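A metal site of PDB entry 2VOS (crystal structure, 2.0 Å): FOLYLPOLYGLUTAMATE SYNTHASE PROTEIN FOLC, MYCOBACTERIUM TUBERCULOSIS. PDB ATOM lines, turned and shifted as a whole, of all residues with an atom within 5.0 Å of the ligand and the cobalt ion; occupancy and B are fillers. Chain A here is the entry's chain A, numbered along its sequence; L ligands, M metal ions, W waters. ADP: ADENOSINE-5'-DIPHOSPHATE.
Water W3 lies within hydrogen-bond range of an oxygen (O1A) of the ligand (2.8 Å) and the guanidinium group (NH2) of Arg 338 (2.9 Å). Water W7 lies within hydrogen-bond range of the backbone carbonyl oxygen (O) of Thr 72 and an oxygen (O2B) of the ligand. Water W1 lies within hydrogen-bond range of the backbone NH of His 354 (2.9 Å), the side-chain amide nitrogen of Asn 73 (3.1 Å) and an oxygen (O4') of the ligand (3.5 Å).
Merely in contact with the cobalt ion: Pro 99 (3.97 Å). The nearest printed residue that does not touch the cobalt ion is Lys 75 (4.5 Å).
The backbone NH (N) of Leu 339 lies within hydrogen-bond range of the side-chain carboxylate (OD1) of Asp 351 (2.7 Å). N of Asn 73 lies within hydrogen-bond range of O of Pro 196 (3.2 Å). N of Ala 352 lies within hydrogen-bond range of O of Gly 337, at 2.9 Å. NZ of Lys 75 lies within hydrogen-bond range of O of Gly 71, at 3.0 Å. The backbone NH (N) of Thr 72 sits at hydrogen-bond distance from the backbone carbonyl oxygen (O) of Pro 196 (3.0 Å). The side-chain carboxylate of Asp 351 sits at hydrogen-bond distance from the backbone NH of Ala 353, 3.0 Å away. O of Ala 352 lies within hydrogen-bond range of ND1 of His 354 (2.9 Å). The side-chain hydroxyl (OG) of Ser 77 lies within hydrogen-bond range of the side-chain hydroxyl (OG) of Ser 335.
The cobalt ion is bound by an oxygen (O1B) of the ligand. Water W3 is bound to the cobalt ion (2.1 Å). The cobalt ion is bound by water W2. OE2 of Glu 174 is bound to the cobalt ion (2.2 Å). OG1 of Thr 76 is bound to the cobalt ion (2.2 Å). The cobalt ion is bound by O of Ser 98, 2.2 Å away.
The side-chain amide nitrogen (ND2) of Asn 73 sits at hydrogen-bond distance from an oxygen (O4') of the ligand (3.2 Å). The side-chain hydroxyl of Ser 77 sits at hydrogen-bond distance from an oxygen (O2A) of the ligand (2.8 Å). The backbone NH (N) of Gly 74 lies within hydrogen-bond range of an oxygen (O3A) of the ligand, 2.9 Å away. N of Lys 75 is in hydrogen-bond range of O3B of the ligand, at 2.8 Å. A nitrogen (N6) of the ligand is in hydrogen-bond range of the side-chain amide oxygen (OD1) of Asn 301. An oxygen (O1B) of the ligand lies close to the backbone NH (N) of Thr 76. O of Gly 358 sits at hydrogen-bond distance from O2' of the ligand, at 3.4 Å. OD2 of Asp 351 lies within hydrogen-bond range of O2' of the ligand (2.9 Å). The backbone NH of Ala 352 is in hydrogen-bond range of an oxygen (O3') of the ligand, 3.5 Å away. The side-chain amino group of Lys 75 is in salt-bridge range of an oxygen (O3B) of the ligand (2.8 Å). O2A of the ligand is in hydrogen-bond range of N of Ser 77 (3.0 Å). O1A of the ligand is in salt-bridge range of NH2 of Arg 338.
O3B of the ligand sits close to O of Thr 72. Merely in contact with the ligand: His 297 (3.6 Å), Ala 353 (3.5 Å), Ala 357 (3.9 Å) and Ala 361 (3.6 Å). Hydrophobic or aromatic side chains within 4 Å of the ligand: His 297, Ala 352, Ala 353 and Ala 361. The nearest printed residue that does not touch the ligand is Pro 196 (4.04 Å).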
ATOM      1  N   GLY A  71     -24.888  22.934   0.205  1.00  0.00           N
ATOM      2  CA  GLY A  71     -24.006  22.126  -0.627  1.00  0.00           C
ATOM      3  C   GLY A  71     -22.878  23.001  -1.082  1.00  0.00           C
ATOM      4  O   GLY A  71     -22.806  24.170  -0.676  1.00  0.00           O
ATOM      5  N   THR A  72     -22.002  22.489  -1.951  1.00  0.00           N
ATOM      6  CA  THR A  72     -20.878  23.280  -2.394  1.00  0.00           C
ATOM      7  C   THR A  72     -21.078  23.868  -3.751  1.00  0.00           C
ATOM      8  O   THR A  72     -20.703  25.026  -3.966  1.00  0.00           O
ATOM      9  CB  THR A  72     -19.566  22.446  -2.433  1.00  0.00           C
ATOM     10  OG1 THR A  72     -19.356  21.925  -1.100  1.00  0.00           O
ATOM     11  CG2 THR A  72     -18.409  23.382  -2.747  1.00  0.00           C
ATOM     12  N   ASN A  73     -21.559  23.090  -4.703  1.00  0.00           N
ATOM     13  CA  ASN A  73     -21.782  23.643  -6.032  1.00  0.00           C
ATOM     14  C   ASN A  73     -23.267  23.390  -6.451  1.00  0.00           C
ATOM     15  O   ASN A  73     -23.828  22.371  -6.111  1.00  0.00           O
ATOM     16  CB  ASN A  73     -20.901  22.963  -7.060  1.00  0.00           C
ATOM     17  CG  ASN A  73     -19.445  23.440  -7.017  1.00  0.00           C
ATOM     18  OD1 ASN A  73     -18.629  22.789  -6.397  1.00  0.00           O
ATOM     19  ND2 ASN A  73     -19.114  24.566  -7.721  1.00  0.00           N
ATOM     20  N   GLY A  74     -23.837  24.331  -7.198  1.00  0.00           N
ATOM     21  CA  GLY A  74     -25.190  24.213  -7.727  1.00  0.00           C
ATOM     22  C   GLY A  74     -26.257  24.739  -6.767  1.00  0.00           C
ATOM     23  O   GLY A  74     -27.456  24.623  -7.090  1.00  0.00           O
ATOM     24  N   LYS A  75     -25.908  25.295  -5.613  1.00  0.00           N
ATOM     25  CA  LYS A  75     -27.001  25.734  -4.710  1.00  0.00           C
ATOM     26  C   LYS A  75     -27.899  26.763  -5.396  1.00  0.00           C
ATOM     27  O   LYS A  75     -29.129  26.651  -5.357  1.00  0.00           O
ATOM     28  CB  LYS A  75     -26.565  26.364  -3.361  1.00  0.00           C
ATOM     29  CG  LYS A  75     -25.744  25.415  -2.383  1.00  0.00           C
ATOM     30  CD  LYS A  75     -25.404  26.162  -1.094  1.00  0.00           C
ATOM     31  CE  LYS A  75     -24.354  27.287  -1.338  1.00  0.00           C
ATOM     32  NZ  LYS A  75     -23.137  26.795  -2.099  1.00  0.00           N
ATOM     33  N   THR A  76     -27.288  27.835  -5.887  1.00  0.00           N
ATOM     34  CA  THR A  76     -28.070  28.923  -6.515  1.00  0.00           C
ATOM     35  C   THR A  76     -28.841  28.395  -7.731  1.00  0.00           C
ATOM     36  O   THR A  76     -30.025  28.717  -7.915  1.00  0.00           O
ATOM     37  CB  THR A  76     -27.173  30.138  -6.901  1.00  0.00           C
ATOM     38  OG1 THR A  76     -26.826  30.773  -5.676  1.00  0.00           O
ATOM     39  CG2 THR A  76     -28.025  31.165  -7.719  1.00  0.00           C
ATOM     40  N   SER A  77     -28.160  27.638  -8.574  1.00  0.00           N
ATOM     41  CA  SER A  77     -28.857  27.129  -9.760  1.00  0.00           C
ATOM     42  C   SER A  77     -30.056  26.219  -9.361  1.00  0.00           C
ATOM     43  O   SER A  77     -31.153  26.296  -9.952  1.00  0.00           O
ATOM     44  CB  SER A  77     -27.892  26.304 -10.610  1.00  0.00           C
ATOM     45  OG  SER A  77     -26.960  27.109 -11.305  1.00  0.00           O
ATOM     46  N   SER A  98     -27.652  33.641  -2.687  1.00  0.00           N
ATOM     47  CA  SER A  98     -26.418  34.342  -2.431  1.00  0.00           C
ATOM     48  C   SER A  98     -25.264  33.597  -3.126  1.00  0.00           C
ATOM     49  O   SER A  98     -25.395  32.420  -3.578  1.00  0.00           O
ATOM     50  CB  SER A  98     -26.156  34.527  -0.932  1.00  0.00           C
ATOM     51  OG  SER A  98     -26.147  33.243  -0.353  1.00  0.00           O
ATOM     52  N   PRO A  99     -24.164  34.347  -3.354  1.00  0.00           N
ATOM     53  CA  PRO A  99     -24.112  35.796  -3.173  1.00  0.00           C
ATOM     54  C   PRO A  99     -24.898  36.481  -4.324  1.00  0.00           C
ATOM     55  O   PRO A  99     -25.363  35.791  -5.207  1.00  0.00           O
ATOM     56  CB  PRO A  99     -22.598  36.138  -3.280  1.00  0.00           C
ATOM     57  CG  PRO A  99     -21.891  34.859  -3.639  1.00  0.00           C
ATOM     58  CD  PRO A  99     -22.922  33.759  -3.888  1.00  0.00           C
ATOM     59  N   GLU A 174     -31.607  29.531   0.106  1.00  0.00           N
ATOM     60  CA  GLU A 174     -30.260  29.020  -0.049  1.00  0.00           C
ATOM     61  C   GLU A 174     -29.421  29.383   1.194  1.00  0.00           C
ATOM     62  O   GLU A 174     -29.438  30.517   1.645  1.00  0.00           O
ATOM     63  CB  GLU A 174     -29.604  29.652  -1.279  1.00  0.00           C
ATOM     64  CG  GLU A 174     -28.153  29.355  -1.430  1.00  0.00           C
ATOM     65  CD  GLU A 174     -27.542  29.970  -2.711  1.00  0.00           C
ATOM     66  OE1 GLU A 174     -28.201  30.713  -3.471  1.00  0.00           O
ATOM     67  OE2 GLU A 174     -26.358  29.692  -2.951  1.00  0.00           O
ATOM     68  N   PRO A 196     -24.043  18.735  -4.500  1.00  0.00           N
ATOM     69  CA  PRO A 196     -22.715  18.104  -4.363  1.00  0.00           C
ATOM     70  C   PRO A 196     -21.784  18.889  -3.492  1.00  0.00           C
ATOM     71  O   PRO A 196     -21.649  20.087  -3.635  1.00  0.00           O
ATOM     72  CB  PRO A 196     -22.185  18.055  -5.801  1.00  0.00           C
ATOM     73  CG  PRO A 196     -23.582  17.851  -6.629  1.00  0.00           C
ATOM     74  CD  PRO A 196     -24.424  18.920  -5.914  1.00  0.00           C
ATOM     75  N   HIS A 297     -23.479  19.177 -15.549  1.00  0.00           N
ATOM     76  CA  HIS A 297     -23.795  19.476 -14.149  1.00  0.00           C
ATOM     77  C   HIS A 297     -25.181  20.078 -13.978  1.00  0.00           C
ATOM     78  O   HIS A 297     -25.838  19.848 -12.935  1.00  0.00           O
ATOM     79  CB  HIS A 297     -22.798  20.441 -13.532  1.00  0.00           C
ATOM     80  CG  HIS A 297     -22.617  21.728 -14.303  1.00  0.00           C
ATOM     81  ND1 HIS A 297     -21.979  21.762 -15.526  1.00  0.00           N
ATOM     82  CD2 HIS A 297     -22.869  23.022 -13.970  1.00  0.00           C
ATOM     83  CE1 HIS A 297     -21.940  23.018 -15.960  1.00  0.00           C
ATOM     84  NE2 HIS A 297     -22.415  23.803 -15.001  1.00  0.00           N
ATOM     85  N   GLN A 298     -25.632  20.871 -14.954  1.00  0.00           N
ATOM     86  CA  GLN A 298     -26.990  21.415 -14.840  1.00  0.00           C
ATOM     87  C   GLN A 298     -28.096  20.318 -14.994  1.00  0.00           C
ATOM     88  O   GLN A 298     -29.176  20.463 -14.489  1.00  0.00           O
ATOM     89  CB  GLN A 298     -27.216  22.606 -15.787  1.00  0.00           C
ATOM     90  CG  GLN A 298     -26.270  23.802 -15.449  1.00  0.00           C
ATOM     91  CD  GLN A 298     -26.652  24.505 -14.151  1.00  0.00           C
ATOM     92  OE1 GLN A 298     -27.529  24.060 -13.420  1.00  0.00           O
ATOM     93  NE2 GLN A 298     -26.039  25.651 -13.894  1.00  0.00           N
ATOM     94  N   ASN A 301     -28.317  19.107 -11.420  1.00  0.00           N
ATOM     95  CA  ASN A 301     -29.024  20.121 -10.641  1.00  0.00           C
ATOM     96  C   ASN A 301     -30.531  20.046 -10.977  1.00  0.00           C
ATOM     97  O   ASN A 301     -31.344  20.111 -10.074  1.00  0.00           O
ATOM     98  CB  ASN A 301     -28.547  21.554 -10.964  1.00  0.00           C
ATOM     99  CG  ASN A 301     -27.105  21.794 -10.506  1.00  0.00           C
ATOM    100  OD1 ASN A 301     -26.589  21.022  -9.685  1.00  0.00           O
ATOM    101  ND2 ASN A 301     -26.481  22.867 -10.985  1.00  0.00           N
ATOM    102  N   SER A 335     -30.116  30.980 -15.100  1.00  0.00           N
ATOM    103  CA  SER A 335     -29.127  31.005 -14.002  1.00  0.00           C
ATOM    104  C   SER A 335     -28.017  32.006 -14.424  1.00  0.00           C
ATOM    105  O   SER A 335     -27.021  31.630 -15.003  1.00  0.00           O
ATOM    106  CB  SER A 335     -28.574  29.613 -13.718  1.00  0.00           C
ATOM    107  OG  SER A 335     -27.833  29.627 -12.474  1.00  0.00           O
ATOM    108  N   GLY A 337     -25.004  34.352 -14.967  1.00  0.00           N
ATOM    109  CA  GLY A 337     -23.599  34.175 -14.592  1.00  0.00           C
ATOM    110  C   GLY A 337     -23.184  32.746 -14.437  1.00  0.00           C
ATOM    111  O   GLY A 337     -22.082  32.522 -13.948  1.00  0.00           O
ATOM    112  N   ARG A 338     -24.015  31.749 -14.806  1.00  0.00           N
ATOM    113  CA  ARG A 338     -23.542  30.331 -14.880  1.00  0.00           C
ATOM    114  C   ARG A 338     -23.515  29.884 -16.349  1.00  0.00           C
ATOM    115  O   ARG A 338     -24.557  29.625 -16.991  1.00  0.00           O
ATOM    116  CB  ARG A 338     -24.428  29.373 -14.051  1.00  0.00           C
ATOM    117  CG  ARG A 338     -24.168  29.480 -12.510  1.00  0.00           C
ATOM    118  CD  ARG A 338     -24.316  30.914 -12.040  1.00  0.00           C
ATOM    119  NE  ARG A 338     -24.315  31.073 -10.583  1.00  0.00           N
ATOM    120  CZ  ARG A 338     -24.481  32.242  -9.934  1.00  0.00           C
ATOM    121  NH1 ARG A 338     -24.653  33.396 -10.582  1.00  0.00           N
ATOM    122  NH2 ARG A 338     -24.459  32.275  -8.624  1.00  0.00           N
ATOM    123  N   LEU A 339     -22.294  29.881 -16.896  1.00  0.00           N
ATOM    124  CA  LEU A 339     -22.064  29.622 -18.302  1.00  0.00           C
ATOM    125  C   LEU A 339     -23.065  30.374 -19.164  1.00  0.00           C
ATOM    126  O   LEU A 339     -23.778  29.778 -20.006  1.00  0.00           O
ATOM    127  CB  LEU A 339     -22.177  28.129 -18.567  1.00  0.00           C
ATOM    128  CG  LEU A 339     -21.042  27.264 -19.164  1.00  0.00           C
ATOM    129  CD1 LEU A 339     -19.851  27.970 -19.704  1.00  0.00           C
ATOM    130  CD2 LEU A 339     -20.763  26.108 -18.209  1.00  0.00           C
ATOM    131  N   ASP A 351     -18.985  33.056 -16.188  1.00  0.00           N
ATOM    132  CA  ASP A 351     -19.211  31.928 -15.325  1.00  0.00           C
ATOM    133  C   ASP A 351     -18.637  32.193 -13.936  1.00  0.00           C
ATOM    134  O   ASP A 351     -17.475  32.593 -13.795  1.00  0.00           O
ATOM    135  CB  ASP A 351     -18.657  30.632 -15.917  1.00  0.00           C
ATOM    136  CG  ASP A 351     -19.184  29.399 -15.148  1.00  0.00           C
ATOM    137  OD1 ASP A 351     -20.310  28.945 -15.348  1.00  0.00           O
ATOM    138  OD2 ASP A 351     -18.507  28.932 -14.263  1.00  0.00           O
ATOM    139  N   ALA A 352     -19.455  31.945 -12.908  1.00  0.00           N
ATOM    140  CA  ALA A 352     -19.100  32.224 -11.533  1.00  0.00           C
ATOM    141  C   ALA A 352     -18.100  31.179 -10.945  1.00  0.00           C
ATOM    142  O   ALA A 352     -17.756  31.292  -9.754  1.00  0.00           O
ATOM    143  CB  ALA A 352     -20.359  32.233 -10.659  1.00  0.00           C
ATOM    144  N   ALA A 353     -17.654  30.179 -11.720  1.00  0.00           N
ATOM    145  CA  ALA A 353     -16.791  29.131 -11.164  1.00  0.00           C
ATOM    146  C   ALA A 353     -15.701  29.718 -10.274  1.00  0.00           C
ATOM    147  O   ALA A 353     -14.967  30.626 -10.677  1.00  0.00           O
ATOM    148  CB  ALA A 353     -16.156  28.306 -12.271  1.00  0.00           C
ATOM    149  N   HIS A 354     -15.586  29.191  -9.060  1.00  0.00           N
ATOM    150  CA  HIS A 354     -14.631  29.713  -8.089  1.00  0.00           C
ATOM    151  C   HIS A 354     -14.120  28.567  -7.177  1.00  0.00           C
ATOM    152  O   HIS A 354     -13.645  28.817  -6.028  1.00  0.00           O
ATOM    153  CB  HIS A 354     -15.240  30.827  -7.253  1.00  0.00           C
ATOM    154  CG  HIS A 354     -16.439  30.394  -6.486  1.00  0.00           C
ATOM    155  ND1 HIS A 354     -17.714  30.623  -6.936  1.00  0.00           N
ATOM    156  CD2 HIS A 354     -16.555  29.716  -5.335  1.00  0.00           C
ATOM    157  CE1 HIS A 354     -18.574  30.140  -6.068  1.00  0.00           C
ATOM    158  NE2 HIS A 354     -17.894  29.580  -5.086  1.00  0.00           N
ATOM    159  N   ALA A 357     -14.147  21.883  -8.487  1.00  0.00           N
ATOM    160  CA  ALA A 357     -15.327  21.238  -9.067  1.00  0.00           C
ATOM    161  C   ALA A 357     -16.075  22.125 -10.108  1.00  0.00           C
ATOM    162  O   ALA A 357     -16.427  21.629 -11.180  1.00  0.00           O
ATOM    163  CB  ALA A 357     -16.300  20.757  -8.004  1.00  0.00           C
ATOM    164  N   GLY A 358     -16.326  23.410  -9.793  1.00  0.00           N
ATOM    165  CA  GLY A 358     -16.987  24.285 -10.740  1.00  0.00           C
ATOM    166  C   GLY A 358     -16.114  24.583 -11.974  1.00  0.00           C
ATOM    167  O   GLY A 358     -16.641  24.654 -13.098  1.00  0.00           O
ATOM    168  N   ALA A 361     -16.330  21.683 -14.164  1.00  0.00           N
ATOM    169  CA  ALA A 361     -17.639  21.576 -14.867  1.00  0.00           C
ATOM    170  C   ALA A 361     -17.650  22.544 -16.062  1.00  0.00           C
ATOM    171  O   ALA A 361     -18.072  22.187 -17.183  1.00  0.00           O
ATOM    172  CB  ALA A 361     -18.772  21.894 -13.935  1.00  0.00           C
ATOM    173  N   LEU A 362     -17.136  23.753 -15.824  1.00  0.00           N
ATOM    174  CA  LEU A 362     -16.972  24.741 -16.845  1.00  0.00           C
ATOM    175  C   LEU A 362     -16.092  24.233 -18.013  1.00  0.00           C
ATOM    176  O   LEU A 362     -16.476  24.358 -19.201  1.00  0.00           O
ATOM    177  CB  LEU A 362     -16.379  26.033 -16.235  1.00  0.00           C
ATOM    178  CG  LEU A 362     -15.965  27.162 -17.163  1.00  0.00           C
ATOM    179  CD1 LEU A 362     -17.118  27.616 -18.148  1.00  0.00           C
ATOM    180  CD2 LEU A 362     -15.414  28.401 -16.344  1.00  0.00           C
HETATM  181  PB  ADP L   1     -23.530  27.781  -5.509  1.00  0.00           P
HETATM  182  O1B ADP L   1     -24.768  28.599  -5.261  1.00  0.00           O
HETATM  183  O2B ADP L   1     -22.253  28.567  -5.364  1.00  0.00           O
HETATM  184  O3B ADP L   1     -23.468  26.434  -4.845  1.00  0.00           O
HETATM  185  PA  ADP L   1     -24.125  28.024  -8.402  1.00  0.00           P
HETATM  186  O1A ADP L   1     -24.051  29.527  -8.214  1.00  0.00           O
HETATM  187  O2A ADP L   1     -25.238  27.278  -9.127  1.00  0.00           O
HETATM  188  O3A ADP L   1     -23.604  27.262  -7.049  1.00  0.00           O
HETATM  189  O5' ADP L   1     -22.838  27.731  -9.346  1.00  0.00           O
HETATM  190  C5' ADP L   1     -21.537  28.327  -9.175  1.00  0.00           C
HETATM  191  C4' ADP L   1     -20.642  27.690 -10.272  1.00  0.00           C
HETATM  192  O4' ADP L   1     -20.497  26.269  -9.984  1.00  0.00           O
HETATM  193  C3' ADP L   1     -21.264  27.677 -11.667  1.00  0.00           C
HETATM  194  O3' ADP L   1     -20.774  28.741 -12.450  1.00  0.00           O
HETATM  195  C2' ADP L   1     -20.824  26.420 -12.370  1.00  0.00           C
HETATM  196  O2' ADP L   1     -19.436  26.653 -12.805  1.00  0.00           O
HETATM  197  C1' ADP L   1     -20.613  25.488 -11.212  1.00  0.00           C
HETATM  198  N9  ADP L   1     -21.719  24.535 -10.907  1.00  0.00           N
HETATM  199  C8  ADP L   1     -23.058  24.737 -10.673  1.00  0.00           C
HETATM  200  N7  ADP L   1     -23.662  23.551 -10.381  1.00  0.00           N
HETATM  201  C5  ADP L   1     -22.674  22.611 -10.320  1.00  0.00           C
HETATM  202  C6  ADP L   1     -22.588  21.178 -10.019  1.00  0.00           C
HETATM  203  N6  ADP L   1     -23.690  20.463  -9.707  1.00  0.00           N
HETATM  204  N1  ADP L   1     -21.377  20.616 -10.135  1.00  0.00           N
HETATM  205  C2  ADP L   1     -20.230  21.237 -10.494  1.00  0.00           C
HETATM  206  N3  ADP L   1     -20.210  22.577 -10.747  1.00  0.00           N
HETATM  207  C4  ADP L   1     -21.406  23.258 -10.684  1.00  0.00           C
HETATM  208 CO    CO M   1     -25.027  30.442  -4.475  1.00  0.00          CO
HETATM  209 MG    MG M   2     -18.839  28.652  -3.524  1.00  0.00          MG
HETATM  210  O   HOH W   1     -17.657  27.274  -8.296  1.00  0.00           O
HETATM  211  O   HOH W   2     -23.340  30.309  -3.140  1.00  0.00           O
HETATM  212  O   HOH W   3     -23.817  31.235  -6.010  1.00  0.00           O
HETATM  213  O   HOH W   4     -23.268  17.330 -10.412  1.00  0.00           O
HETATM  214  O   HOH W   5     -21.533  30.931  -5.297  1.00  0.00           O
HETATM  215  O   HOH W   6     -20.493  18.133  -9.134  1.00  0.00           O
HETATM  216  O   HOH W   7     -19.791  27.298  -5.205  1.00  0.00           O
